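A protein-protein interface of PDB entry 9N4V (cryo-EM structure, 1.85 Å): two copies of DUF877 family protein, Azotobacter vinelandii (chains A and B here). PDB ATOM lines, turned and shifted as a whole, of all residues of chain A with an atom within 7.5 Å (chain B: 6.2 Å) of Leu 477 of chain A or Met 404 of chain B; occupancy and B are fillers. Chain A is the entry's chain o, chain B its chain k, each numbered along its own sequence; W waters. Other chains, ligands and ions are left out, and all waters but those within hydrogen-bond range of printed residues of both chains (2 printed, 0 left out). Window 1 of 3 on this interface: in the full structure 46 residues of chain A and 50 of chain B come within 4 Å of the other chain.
Leu 477 of chain A touches three residues of chain B. Of chain A, only Leu 474 (3.7 Å) and Leu 477 (3.5 Å) come within 4 Å of Met 404 of chain B. Of the printed residues of chain A, Tyr 462 of chain B touches Leu 474 (3.4 Å), Glu 476 (3.1 Å), Leu 477 (3.3 Å) and Thr 478 (3.0 Å). Printed residues of chain B within 4 Å of Ser 480 of chain A: Ala 464. Of the printed residues of chain A, Gly 460 of chain B touches Leu 474, Glu 475 and Glu 476. Tyr 399 of chain B touches none of the printed residues of chain A. Ile 403 of chain B touches none of the printed residues of chain A.
Water W1 lies within hydrogen-bond range of O of Tyr 462 of chain B (2.9 Å) and OG1 of Thr 478 of chain A (3.1 Å). Water W2 lies within hydrogen-bond range of O of Ala 464 of chain B (3.1 Å), O of Thr 478 of chain A (3.2 Å), NH2 of Arg 463 of chain B (3.3 Å) and N of Ser 480 of chain A (3.5 Å).
Of the 8 printed residues of chain A, 8 touch a printed residue of chain B. Hydrophobic or aromatic side chains of chain A that line the printed part of chain B: Phe 361, Leu 474, Leu 477 and Ala 479. Printed residues of chain B that touch a printed residue of chain A: Leu 400, Met 404, Arg 405, Lys 407, Val 408, Gly 460, Val 461, Tyr 462, Arg 463 and Ala 464. Along chain B the printed residues that touch a printed residue of chain A span positions 400 to 464. Among the printed residues, 20 pairs touch across the chains. Among the printed residues, no Asp or Glu carboxylate lies within 4 Å of a Lys or Arg side-chain nitrogen of the other chain.
No position is printed for both chains. Of the 20 pairs that touch across the chains among the printed residues, none has its exchanged pair printed and touching as well.
The backbone carbonyl oxygen of Gly 460 of chain B sits at hydrogen-bond distance from the backbone NH of Glu 475 of chain A. O of Gly 460 of chain B sits at hydrogen-bond distance from N of Glu 476 of chain A. The backbone NH of Tyr 462 of chain B lies within hydrogen-bond range of the backbone carbonyl oxygen of Glu 476 of chain A (3.1 Å). The backbone NH (N) of Thr 478 of chain A sits at hydrogen-bond distance from the backbone carbonyl oxygen (O) of Tyr 462 of chain B. N of Ala 464 of chain B sits at hydrogen-bond distance from O of Thr 478 of chain A, at 2.8 Å. The backbone carbonyl oxygen (O) of Ala 464 of chain B lies within hydrogen-bond range of the backbone NH (N) of Ser 480 of chain A (2.9 Å).
Phe 361 of chain A touches Arg 405 of chain B (CE1 to O, 3.5 Å). Leu 474 of chain A touches Met 404 of chain B. Lys 407 of chain B touches Leu 474 of chain A (O to CD2, 3.4 Å). N of Val 408 of chain B touches CD2 of Leu 474 of chain A, at 3.8 Å. O of Gly 460 of chain B touches C of Leu 474 of chain A (3.7 Å). Tyr 462 of chain B touches Leu 474 of chain A (CD2 to CD1, 3.4 Å). Met 404 of chain B touches Leu 477 of chain A (CG to CD2, 3.5 Å). CB of Ala 464 of chain B touches CD1 of Leu 477 of chain A (3.96 Å). O of Thr 478 of chain A touches CA of Arg 463 of chain B, 3.2 Å away. Ala 464 of chain B touches Ala 479 of chain A (O to CA, 3.2 Å).
The side-chain hydroxyl (OH) of Tyr 462 of chain B is in hydrogen-bond range of the backbone carbonyl oxygen (O) of Met 412 of chain B, at 2.7 Å.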
ATOM      1  N   PHE A 361      -5.445  -4.628  27.175  1.00  0.00           N
ATOM      2  CA  PHE A 361      -4.062  -4.247  26.893  1.00  0.00           C
ATOM      3  C   PHE A 361      -3.830  -4.037  25.401  1.00  0.00           C
ATOM      4  O   PHE A 361      -3.145  -3.091  25.001  1.00  0.00           O
ATOM      5  CB  PHE A 361      -3.099  -5.293  27.445  1.00  0.00           C
ATOM      6  CG  PHE A 361      -2.902  -5.203  28.927  1.00  0.00           C
ATOM      7  CD1 PHE A 361      -2.140  -4.187  29.481  1.00  0.00           C
ATOM      8  CD2 PHE A 361      -3.500  -6.123  29.769  1.00  0.00           C
ATOM      9  CE1 PHE A 361      -1.971  -4.103  30.849  1.00  0.00           C
ATOM     10  CE2 PHE A 361      -3.332  -6.042  31.136  1.00  0.00           C
ATOM     11  CZ  PHE A 361      -2.569  -5.032  31.675  1.00  0.00           C
ATOM     12  N   LEU A 474       2.634   2.231  23.049  1.00  0.00           N
ATOM     13  CA  LEU A 474       3.617   1.221  23.418  1.00  0.00           C
ATOM     14  C   LEU A 474       3.031  -0.177  23.281  1.00  0.00           C
ATOM     15  O   LEU A 474       1.956  -0.466  23.809  1.00  0.00           O
ATOM     16  CB  LEU A 474       4.098   1.449  24.851  1.00  0.00           C
ATOM     17  CG  LEU A 474       4.971   0.348  25.453  1.00  0.00           C
ATOM     18  CD1 LEU A 474       6.330   0.332  24.785  1.00  0.00           C
ATOM     19  CD2 LEU A 474       5.103   0.517  26.962  1.00  0.00           C
ATOM     20  N   GLU A 475       3.757  -1.053  22.587  1.00  0.00           N
ATOM     21  CA  GLU A 475       3.316  -2.418  22.336  1.00  0.00           C
ATOM     22  C   GLU A 475       4.130  -3.461  23.089  1.00  0.00           C
ATOM     23  O   GLU A 475       3.556  -4.346  23.721  1.00  0.00           O
ATOM     24  CB  GLU A 475       3.363  -2.725  20.829  1.00  0.00           C
ATOM     25  CG  GLU A 475       2.493  -1.817  19.978  1.00  0.00           C
ATOM     26  CD  GLU A 475       1.023  -2.193  20.027  1.00  0.00           C
ATOM     27  OE1 GLU A 475       0.681  -3.210  20.661  1.00  0.00           O
ATOM     28  OE2 GLU A 475       0.203  -1.464  19.431  1.00  0.00           O
ATOM     29  N   GLU A 476       5.455  -3.391  23.025  1.00  0.00           N
ATOM     30  CA  GLU A 476       6.319  -4.399  23.621  1.00  0.00           C
ATOM     31  C   GLU A 476       7.604  -3.743  24.097  1.00  0.00           C
ATOM     32  O   GLU A 476       8.028  -2.712  23.574  1.00  0.00           O
ATOM     33  CB  GLU A 476       6.672  -5.526  22.636  1.00  0.00           C
ATOM     34  CG  GLU A 476       5.502  -6.259  22.018  1.00  0.00           C
ATOM     35  CD  GLU A 476       5.919  -7.113  20.833  1.00  0.00           C
ATOM     36  OE1 GLU A 476       7.064  -7.606  20.827  1.00  0.00           O
ATOM     37  OE2 GLU A 476       5.105  -7.284  19.903  1.00  0.00           O
ATOM     38  N   LEU A 477       8.233  -4.370  25.088  1.00  0.00           N
ATOM     39  CA  LEU A 477       9.545  -3.940  25.557  1.00  0.00           C
ATOM     40  C   LEU A 477      10.342  -5.167  25.963  1.00  0.00           C
ATOM     41  O   LEU A 477       9.887  -5.952  26.796  1.00  0.00           O
ATOM     42  CB  LEU A 477       9.434  -2.963  26.729  1.00  0.00           C
ATOM     43  CG  LEU A 477      10.784  -2.586  27.349  1.00  0.00           C
ATOM     44  CD1 LEU A 477      11.539  -1.622  26.458  1.00  0.00           C
ATOM     45  CD2 LEU A 477      10.620  -2.010  28.743  1.00  0.00           C
ATOM     46  N   THR A 478      11.514  -5.337  25.366  1.00  0.00           N
ATOM     47  CA  THR A 478      12.455  -6.380  25.752  1.00  0.00           C
ATOM     48  C   THR A 478      13.624  -5.710  26.457  1.00  0.00           C
ATOM     49  O   THR A 478      14.284  -4.844  25.877  1.00  0.00           O
ATOM     50  CB  THR A 478      12.941  -7.176  24.539  1.00  0.00           C
ATOM     51  OG1 THR A 478      11.833  -7.834  23.916  1.00  0.00           O
ATOM     52  CG2 THR A 478      13.968  -8.217  24.964  1.00  0.00           C
ATOM     53  N   ALA A 479      13.878  -6.102  27.698  1.00  0.00           N
ATOM     54  CA  ALA A 479      14.884  -5.448  28.519  1.00  0.00           C
ATOM     55  C   ALA A 479      15.933  -6.446  28.985  1.00  0.00           C
ATOM     56  O   ALA A 479      15.621  -7.601  29.279  1.00  0.00           O
ATOM     57  CB  ALA A 479      14.247  -4.762  29.722  1.00  0.00           C
ATOM     58  N   SER A 480      17.178  -5.988  29.043  1.00  0.00           N
ATOM     59  CA  SER A 480      18.292  -6.763  29.568  1.00  0.00           C
ATOM     60  C   SER A 480      18.878  -6.007  30.752  1.00  0.00           C
ATOM     61  O   SER A 480      19.357  -4.882  30.595  1.00  0.00           O
ATOM     62  CB  SER A 480      19.351  -6.998  28.489  1.00  0.00           C
ATOM     63  OG  SER A 480      20.541  -7.527  29.038  1.00  0.00           O
ATOM     64  N   TYR B 399      10.102  -4.857  39.361  1.00  0.00           N
ATOM     65  CA  TYR B 399       9.580  -3.502  39.236  1.00  0.00           C
ATOM     66  C   TYR B 399       9.398  -3.115  37.777  1.00  0.00           C
ATOM     67  O   TYR B 399       8.381  -2.512  37.409  1.00  0.00           O
ATOM     68  CB  TYR B 399      10.513  -2.516  39.931  1.00  0.00           C
ATOM     69  CG  TYR B 399      10.165  -2.286  41.376  1.00  0.00           C
ATOM     70  CD1 TYR B 399       8.964  -1.689  41.730  1.00  0.00           C
ATOM     71  CD2 TYR B 399      11.029  -2.671  42.389  1.00  0.00           C
ATOM     72  CE1 TYR B 399       8.635  -1.474  43.048  1.00  0.00           C
ATOM     73  CE2 TYR B 399      10.706  -2.464  43.718  1.00  0.00           C
ATOM     74  CZ  TYR B 399       9.509  -1.863  44.039  1.00  0.00           C
ATOM     75  OH  TYR B 399       9.176  -1.650  45.353  1.00  0.00           O
ATOM     76  N   LEU B 400      10.381  -3.438  36.935  1.00  0.00           N
ATOM     77  CA  LEU B 400      10.288  -3.104  35.519  1.00  0.00           C
ATOM     78  C   LEU B 400       9.095  -3.799  34.878  1.00  0.00           C
ATOM     79  O   LEU B 400       8.320  -3.172  34.150  1.00  0.00           O
ATOM     80  CB  LEU B 400      11.584  -3.484  34.810  1.00  0.00           C
ATOM     81  CG  LEU B 400      11.709  -3.015  33.363  1.00  0.00           C
ATOM     82  CD1 LEU B 400      11.665  -1.503  33.286  1.00  0.00           C
ATOM     83  CD2 LEU B 400      12.995  -3.537  32.761  1.00  0.00           C
ATOM     84  N   LYS B 401       8.918  -5.090  35.168  1.00  0.00           N
ATOM     85  CA  LYS B 401       7.758  -5.815  34.664  1.00  0.00           C
ATOM     86  C   LYS B 401       6.468  -5.088  35.023  1.00  0.00           C
ATOM     87  O   LYS B 401       5.652  -4.782  34.149  1.00  0.00           O
ATOM     88  CB  LYS B 401       7.748  -7.240  35.221  1.00  0.00           C
ATOM     89  CG  LYS B 401       6.643  -8.133  34.660  1.00  0.00           C
ATOM     90  CD  LYS B 401       6.795  -8.315  33.155  1.00  0.00           C
ATOM     91  CE  LYS B 401       6.038  -9.531  32.634  1.00  0.00           C
ATOM     92  NZ  LYS B 401       5.921 -10.599  33.645  1.00  0.00           N
ATOM     93  N   VAL B 402       6.298  -4.752  36.302  1.00  0.00           N
ATOM     94  CA  VAL B 402       5.022  -4.194  36.747  1.00  0.00           C
ATOM     95  C   VAL B 402       4.776  -2.810  36.136  1.00  0.00           C
ATOM     96  O   VAL B 402       3.702  -2.540  35.576  1.00  0.00           O
ATOM     97  CB  VAL B 402       4.968  -4.166  38.285  1.00  0.00           C
ATOM     98  CG1 VAL B 402       3.806  -3.323  38.758  1.00  0.00           C
ATOM     99  CG2 VAL B 402       4.854  -5.582  38.814  1.00  0.00           C
ATOM    100  N   ILE B 403       5.769  -1.920  36.200  1.00  0.00           N
ATOM    101  CA  ILE B 403       5.531  -0.550  35.744  1.00  0.00           C
ATOM    102  C   ILE B 403       5.382  -0.493  34.221  1.00  0.00           C
ATOM    103  O   ILE B 403       4.509   0.215  33.695  1.00  0.00           O
ATOM    104  CB  ILE B 403       6.628   0.400  36.265  1.00  0.00           C
ATOM    105  CG1 ILE B 403       7.995   0.090  35.655  1.00  0.00           C
ATOM    106  CG2 ILE B 403       6.703   0.344  37.786  1.00  0.00           C
ATOM    107  CD1 ILE B 403       9.100   1.014  36.131  1.00  0.00           C
ATOM    108  N   MET B 404       6.203  -1.247  33.482  1.00  0.00           N
ATOM    109  CA  MET B 404       6.066  -1.227  32.034  1.00  0.00           C
ATOM    110  C   MET B 404       4.777  -1.904  31.586  1.00  0.00           C
ATOM    111  O   MET B 404       4.180  -1.480  30.592  1.00  0.00           O
ATOM    112  CB  MET B 404       7.285  -1.871  31.377  1.00  0.00           C
ATOM    113  CG  MET B 404       8.532  -0.998  31.422  1.00  0.00           C
ATOM    114  SD  MET B 404       8.211   0.775  31.285  1.00  0.00           S
ATOM    115  CE  MET B 404       7.732   0.924  29.568  1.00  0.00           C
ATOM    116  N   ARG B 405       4.318  -2.935  32.301  1.00  0.00           N
ATOM    117  CA  ARG B 405       2.980  -3.451  32.038  1.00  0.00           C
ATOM    118  C   ARG B 405       1.942  -2.351  32.202  1.00  0.00           C
ATOM    119  O   ARG B 405       0.994  -2.258  31.416  1.00  0.00           O
ATOM    120  CB  ARG B 405       2.669  -4.629  32.964  1.00  0.00           C
ATOM    121  CG  ARG B 405       1.214  -5.069  32.941  1.00  0.00           C
ATOM    122  CD  ARG B 405       0.905  -6.068  34.055  1.00  0.00           C
ATOM    123  NE  ARG B 405       1.634  -7.320  33.901  1.00  0.00           N
ATOM    124  CZ  ARG B 405       2.293  -7.932  34.876  1.00  0.00           C
ATOM    125  NH1 ARG B 405       2.355  -7.424  36.094  1.00  0.00           N
ATOM    126  NH2 ARG B 405       2.898  -9.085  34.622  1.00  0.00           N
ATOM    127  N   ASP B 406       2.117  -1.494  33.212  1.00  0.00           N
ATOM    128  CA  ASP B 406       1.206  -0.363  33.369  1.00  0.00           C
ATOM    129  C   ASP B 406       1.307   0.625  32.208  1.00  0.00           C
ATOM    130  O   ASP B 406       0.356   1.368  31.949  1.00  0.00           O
ATOM    131  CB  ASP B 406       1.476   0.358  34.687  1.00  0.00           C
ATOM    132  CG  ASP B 406       0.696  -0.229  35.842  1.00  0.00           C
ATOM    133  OD1 ASP B 406      -0.078  -1.178  35.616  1.00  0.00           O
ATOM    134  OD2 ASP B 406       0.865   0.255  36.978  1.00  0.00           O
ATOM    135  N   LYS B 407       2.446   0.676  31.519  1.00  0.00           N
ATOM    136  CA  LYS B 407       2.590   1.647  30.435  1.00  0.00           C
ATOM    137  C   LYS B 407       2.213   1.111  29.051  1.00  0.00           C
ATOM    138  O   LYS B 407       2.190   1.890  28.095  1.00  0.00           O
ATOM    139  CB  LYS B 407       4.021   2.184  30.398  1.00  0.00           C
ATOM    140  CG  LYS B 407       4.320   3.203  31.494  1.00  0.00           C
ATOM    141  CD  LYS B 407       3.734   4.564  31.168  1.00  0.00           C
ATOM    142  CE  LYS B 407       3.962   5.575  32.285  1.00  0.00           C
ATOM    143  NZ  LYS B 407       3.457   5.110  33.605  1.00  0.00           N
ATOM    144  N   VAL B 408       1.916  -0.182  28.912  1.00  0.00           N
ATOM    145  CA  VAL B 408       1.502  -0.712  27.615  1.00  0.00           C
ATOM    146  C   VAL B 408       0.216  -0.026  27.170  1.00  0.00           C
ATOM    147  O   VAL B 408      -0.744   0.086  27.938  1.00  0.00           O
ATOM    148  CB  VAL B 408       1.324  -2.235  27.690  1.00  0.00           C
ATOM    149  CG1 VAL B 408       0.490  -2.736  26.515  1.00  0.00           C
ATOM    150  CG2 VAL B 408       2.673  -2.927  27.735  1.00  0.00           C
ATOM    151  N   MET B 412       3.778   6.459  23.685  1.00  0.00           N
ATOM    152  CA  MET B 412       5.164   6.592  24.119  1.00  0.00           C
ATOM    153  C   MET B 412       6.104   6.398  22.943  1.00  0.00           C
ATOM    154  O   MET B 412       5.994   5.409  22.214  1.00  0.00           O
ATOM    155  CB  MET B 412       5.509   5.581  25.217  1.00  0.00           C
ATOM    156  CG  MET B 412       4.594   5.619  26.428  1.00  0.00           C
ATOM    157  SD  MET B 412       5.298   4.785  27.860  1.00  0.00           S
ATOM    158  CE  MET B 412       6.577   5.937  28.358  1.00  0.00           C
ATOM    159  N   VAL B 417      10.032   6.459  26.699  1.00  0.00           N
ATOM    160  CA  VAL B 417      10.332   5.290  27.521  1.00  0.00           C
ATOM    161  C   VAL B 417      11.650   5.487  28.257  1.00  0.00           C
ATOM    162  O   VAL B 417      11.760   5.214  29.459  1.00  0.00           O
ATOM    163  CB  VAL B 417      10.356   4.016  26.657  1.00  0.00           C
ATOM    164  CG1 VAL B 417      10.754   2.810  27.500  1.00  0.00           C
ATOM    165  CG2 VAL B 417       9.005   3.790  25.991  1.00  0.00           C
ATOM    166  N   TYR B 420      11.253   8.091  31.048  1.00  0.00           N
ATOM    167  CA  TYR B 420      10.479   7.556  32.160  1.00  0.00           C
ATOM    168  C   TYR B 420      11.315   6.598  32.999  1.00  0.00           C
ATOM    169  O   TYR B 420      11.363   6.716  34.226  1.00  0.00           O
ATOM    170  CB  TYR B 420       9.220   6.857  31.648  1.00  0.00           C
ATOM    171  CG  TYR B 420       8.456   6.159  32.748  1.00  0.00           C
ATOM    172  CD1 TYR B 420       7.757   6.887  33.698  1.00  0.00           C
ATOM    173  CD2 TYR B 420       8.452   4.776  32.853  1.00  0.00           C
ATOM    174  CE1 TYR B 420       7.067   6.262  34.711  1.00  0.00           C
ATOM    175  CE2 TYR B 420       7.758   4.140  33.864  1.00  0.00           C
ATOM    176  CZ  TYR B 420       7.069   4.892  34.792  1.00  0.00           C
ATOM    177  OH  TYR B 420       6.374   4.274  35.802  1.00  0.00           O
ATOM    178  N   LEU B 421      11.993   5.649  32.351  1.00  0.00           N
ATOM    179  CA  LEU B 421      12.734   4.639  33.101  1.00  0.00           C
ATOM    180  C   LEU B 421      13.916   5.247  33.847  1.00  0.00           C
ATOM    181  O   LEU B 421      14.193   4.865  34.989  1.00  0.00           O
ATOM    182  CB  LEU B 421      13.194   3.522  32.169  1.00  0.00           C
ATOM    183  CG  LEU B 421      12.057   2.597  31.730  1.00  0.00           C
ATOM    184  CD1 LEU B 421      12.574   1.450  30.884  1.00  0.00           C
ATOM    185  CD2 LEU B 421      11.292   2.082  32.939  1.00  0.00           C
ATOM    186  N   VAL B 452      17.455   2.895  25.667  1.00  0.00           N
ATOM    187  CA  VAL B 452      16.309   2.353  24.946  1.00  0.00           C
ATOM    188  C   VAL B 452      16.527   2.544  23.451  1.00  0.00           C
ATOM    189  O   VAL B 452      16.985   3.603  23.011  1.00  0.00           O
ATOM    190  CB  VAL B 452      14.989   3.016  25.391  1.00  0.00           C
ATOM    191  CG1 VAL B 452      13.815   2.430  24.630  1.00  0.00           C
ATOM    192  CG2 VAL B 452      14.788   2.866  26.898  1.00  0.00           C
ATOM    193  N   GLY B 460       6.084   1.208  18.161  1.00  0.00           N
ATOM    194  CA  GLY B 460       5.752   0.934  19.544  1.00  0.00           C
ATOM    195  C   GLY B 460       6.434  -0.268  20.160  1.00  0.00           C
ATOM    196  O   GLY B 460       6.019  -0.702  21.237  1.00  0.00           O
ATOM    197  N   VAL B 461       7.462  -0.821  19.520  1.00  0.00           N
ATOM    198  CA  VAL B 461       8.213  -1.957  20.044  1.00  0.00           C
ATOM    199  C   VAL B 461       9.642  -1.498  20.312  1.00  0.00           C
ATOM    200  O   VAL B 461      10.300  -0.955  19.418  1.00  0.00           O
ATOM    201  CB  VAL B 461       8.186  -3.151  19.071  1.00  0.00           C
ATOM    202  CG1 VAL B 461       9.063  -4.289  19.585  1.00  0.00           C
ATOM    203  CG2 VAL B 461       6.754  -3.618  18.852  1.00  0.00           C
ATOM    204  N   TYR B 462      10.121  -1.721  21.535  1.00  0.00           N
ATOM    205  CA  TYR B 462      11.400  -1.180  21.972  1.00  0.00           C
ATOM    206  C   TYR B 462      12.232  -2.238  22.687  1.00  0.00           C
ATOM    207  O   TYR B 462      11.718  -3.240  23.184  1.00  0.00           O
ATOM    208  CB  TYR B 462      11.209   0.027  22.897  1.00  0.00           C
ATOM    209  CG  TYR B 462      10.297   1.084  22.335  1.00  0.00           C
ATOM    210  CD1 TYR B 462      10.731   1.943  21.336  1.00  0.00           C
ATOM    211  CD2 TYR B 462       8.999   1.217  22.794  1.00  0.00           C
ATOM    212  CE1 TYR B 462       9.897   2.909  20.815  1.00  0.00           C
ATOM    213  CE2 TYR B 462       8.155   2.183  22.282  1.00  0.00           C
ATOM    214  CZ  TYR B 462       8.610   3.026  21.293  1.00  0.00           C
ATOM    215  OH  TYR B 462       7.776   3.985  20.783  1.00  0.00           O
ATOM    216  N   ARG B 463      13.538  -1.995  22.724  1.00  0.00           N
ATOM    217  CA  ARG B 463      14.482  -2.789  23.496  1.00  0.00           C
ATOM    218  C   ARG B 463      15.244  -1.868  24.433  1.00  0.00           C
ATOM    219  O   ARG B 463      15.587  -0.742  24.065  1.00  0.00           O
ATOM    220  CB  ARG B 463      15.464  -3.539  22.596  1.00  0.00           C
ATOM    221  CG  ARG B 463      14.799  -4.384  21.529  1.00  0.00           C
ATOM    222  CD  ARG B 463      15.809  -5.235  20.770  1.00  0.00           C
ATOM    223  NE  ARG B 463      16.767  -5.896  21.647  1.00  0.00           N
ATOM    224  CZ  ARG B 463      16.707  -7.178  21.982  1.00  0.00           C
ATOM    225  NH1 ARG B 463      15.726  -7.955  21.558  1.00  0.00           N
ATOM    226  NH2 ARG B 463      17.653  -7.691  22.761  1.00  0.00           N
ATOM    227  N   ALA B 464      15.509  -2.344  25.641  1.00  0.00           N
ATOM    228  CA  ALA B 464      16.208  -1.546  26.633  1.00  0.00           C
ATOM    229  C   ALA B 464      17.323  -2.359  27.273  1.00  0.00           C
ATOM    230  O   ALA B 464      17.239  -3.582  27.389  1.00  0.00           O
ATOM    231  CB  ALA B 464      15.250  -1.029  27.707  1.00  0.00           C
HETATM  232  O   HOH W   1      11.377  -5.772  21.713  1.00  0.00           O
HETATM  233  O   HOH W   2      17.208  -6.089  25.561  1.00  0.00           O
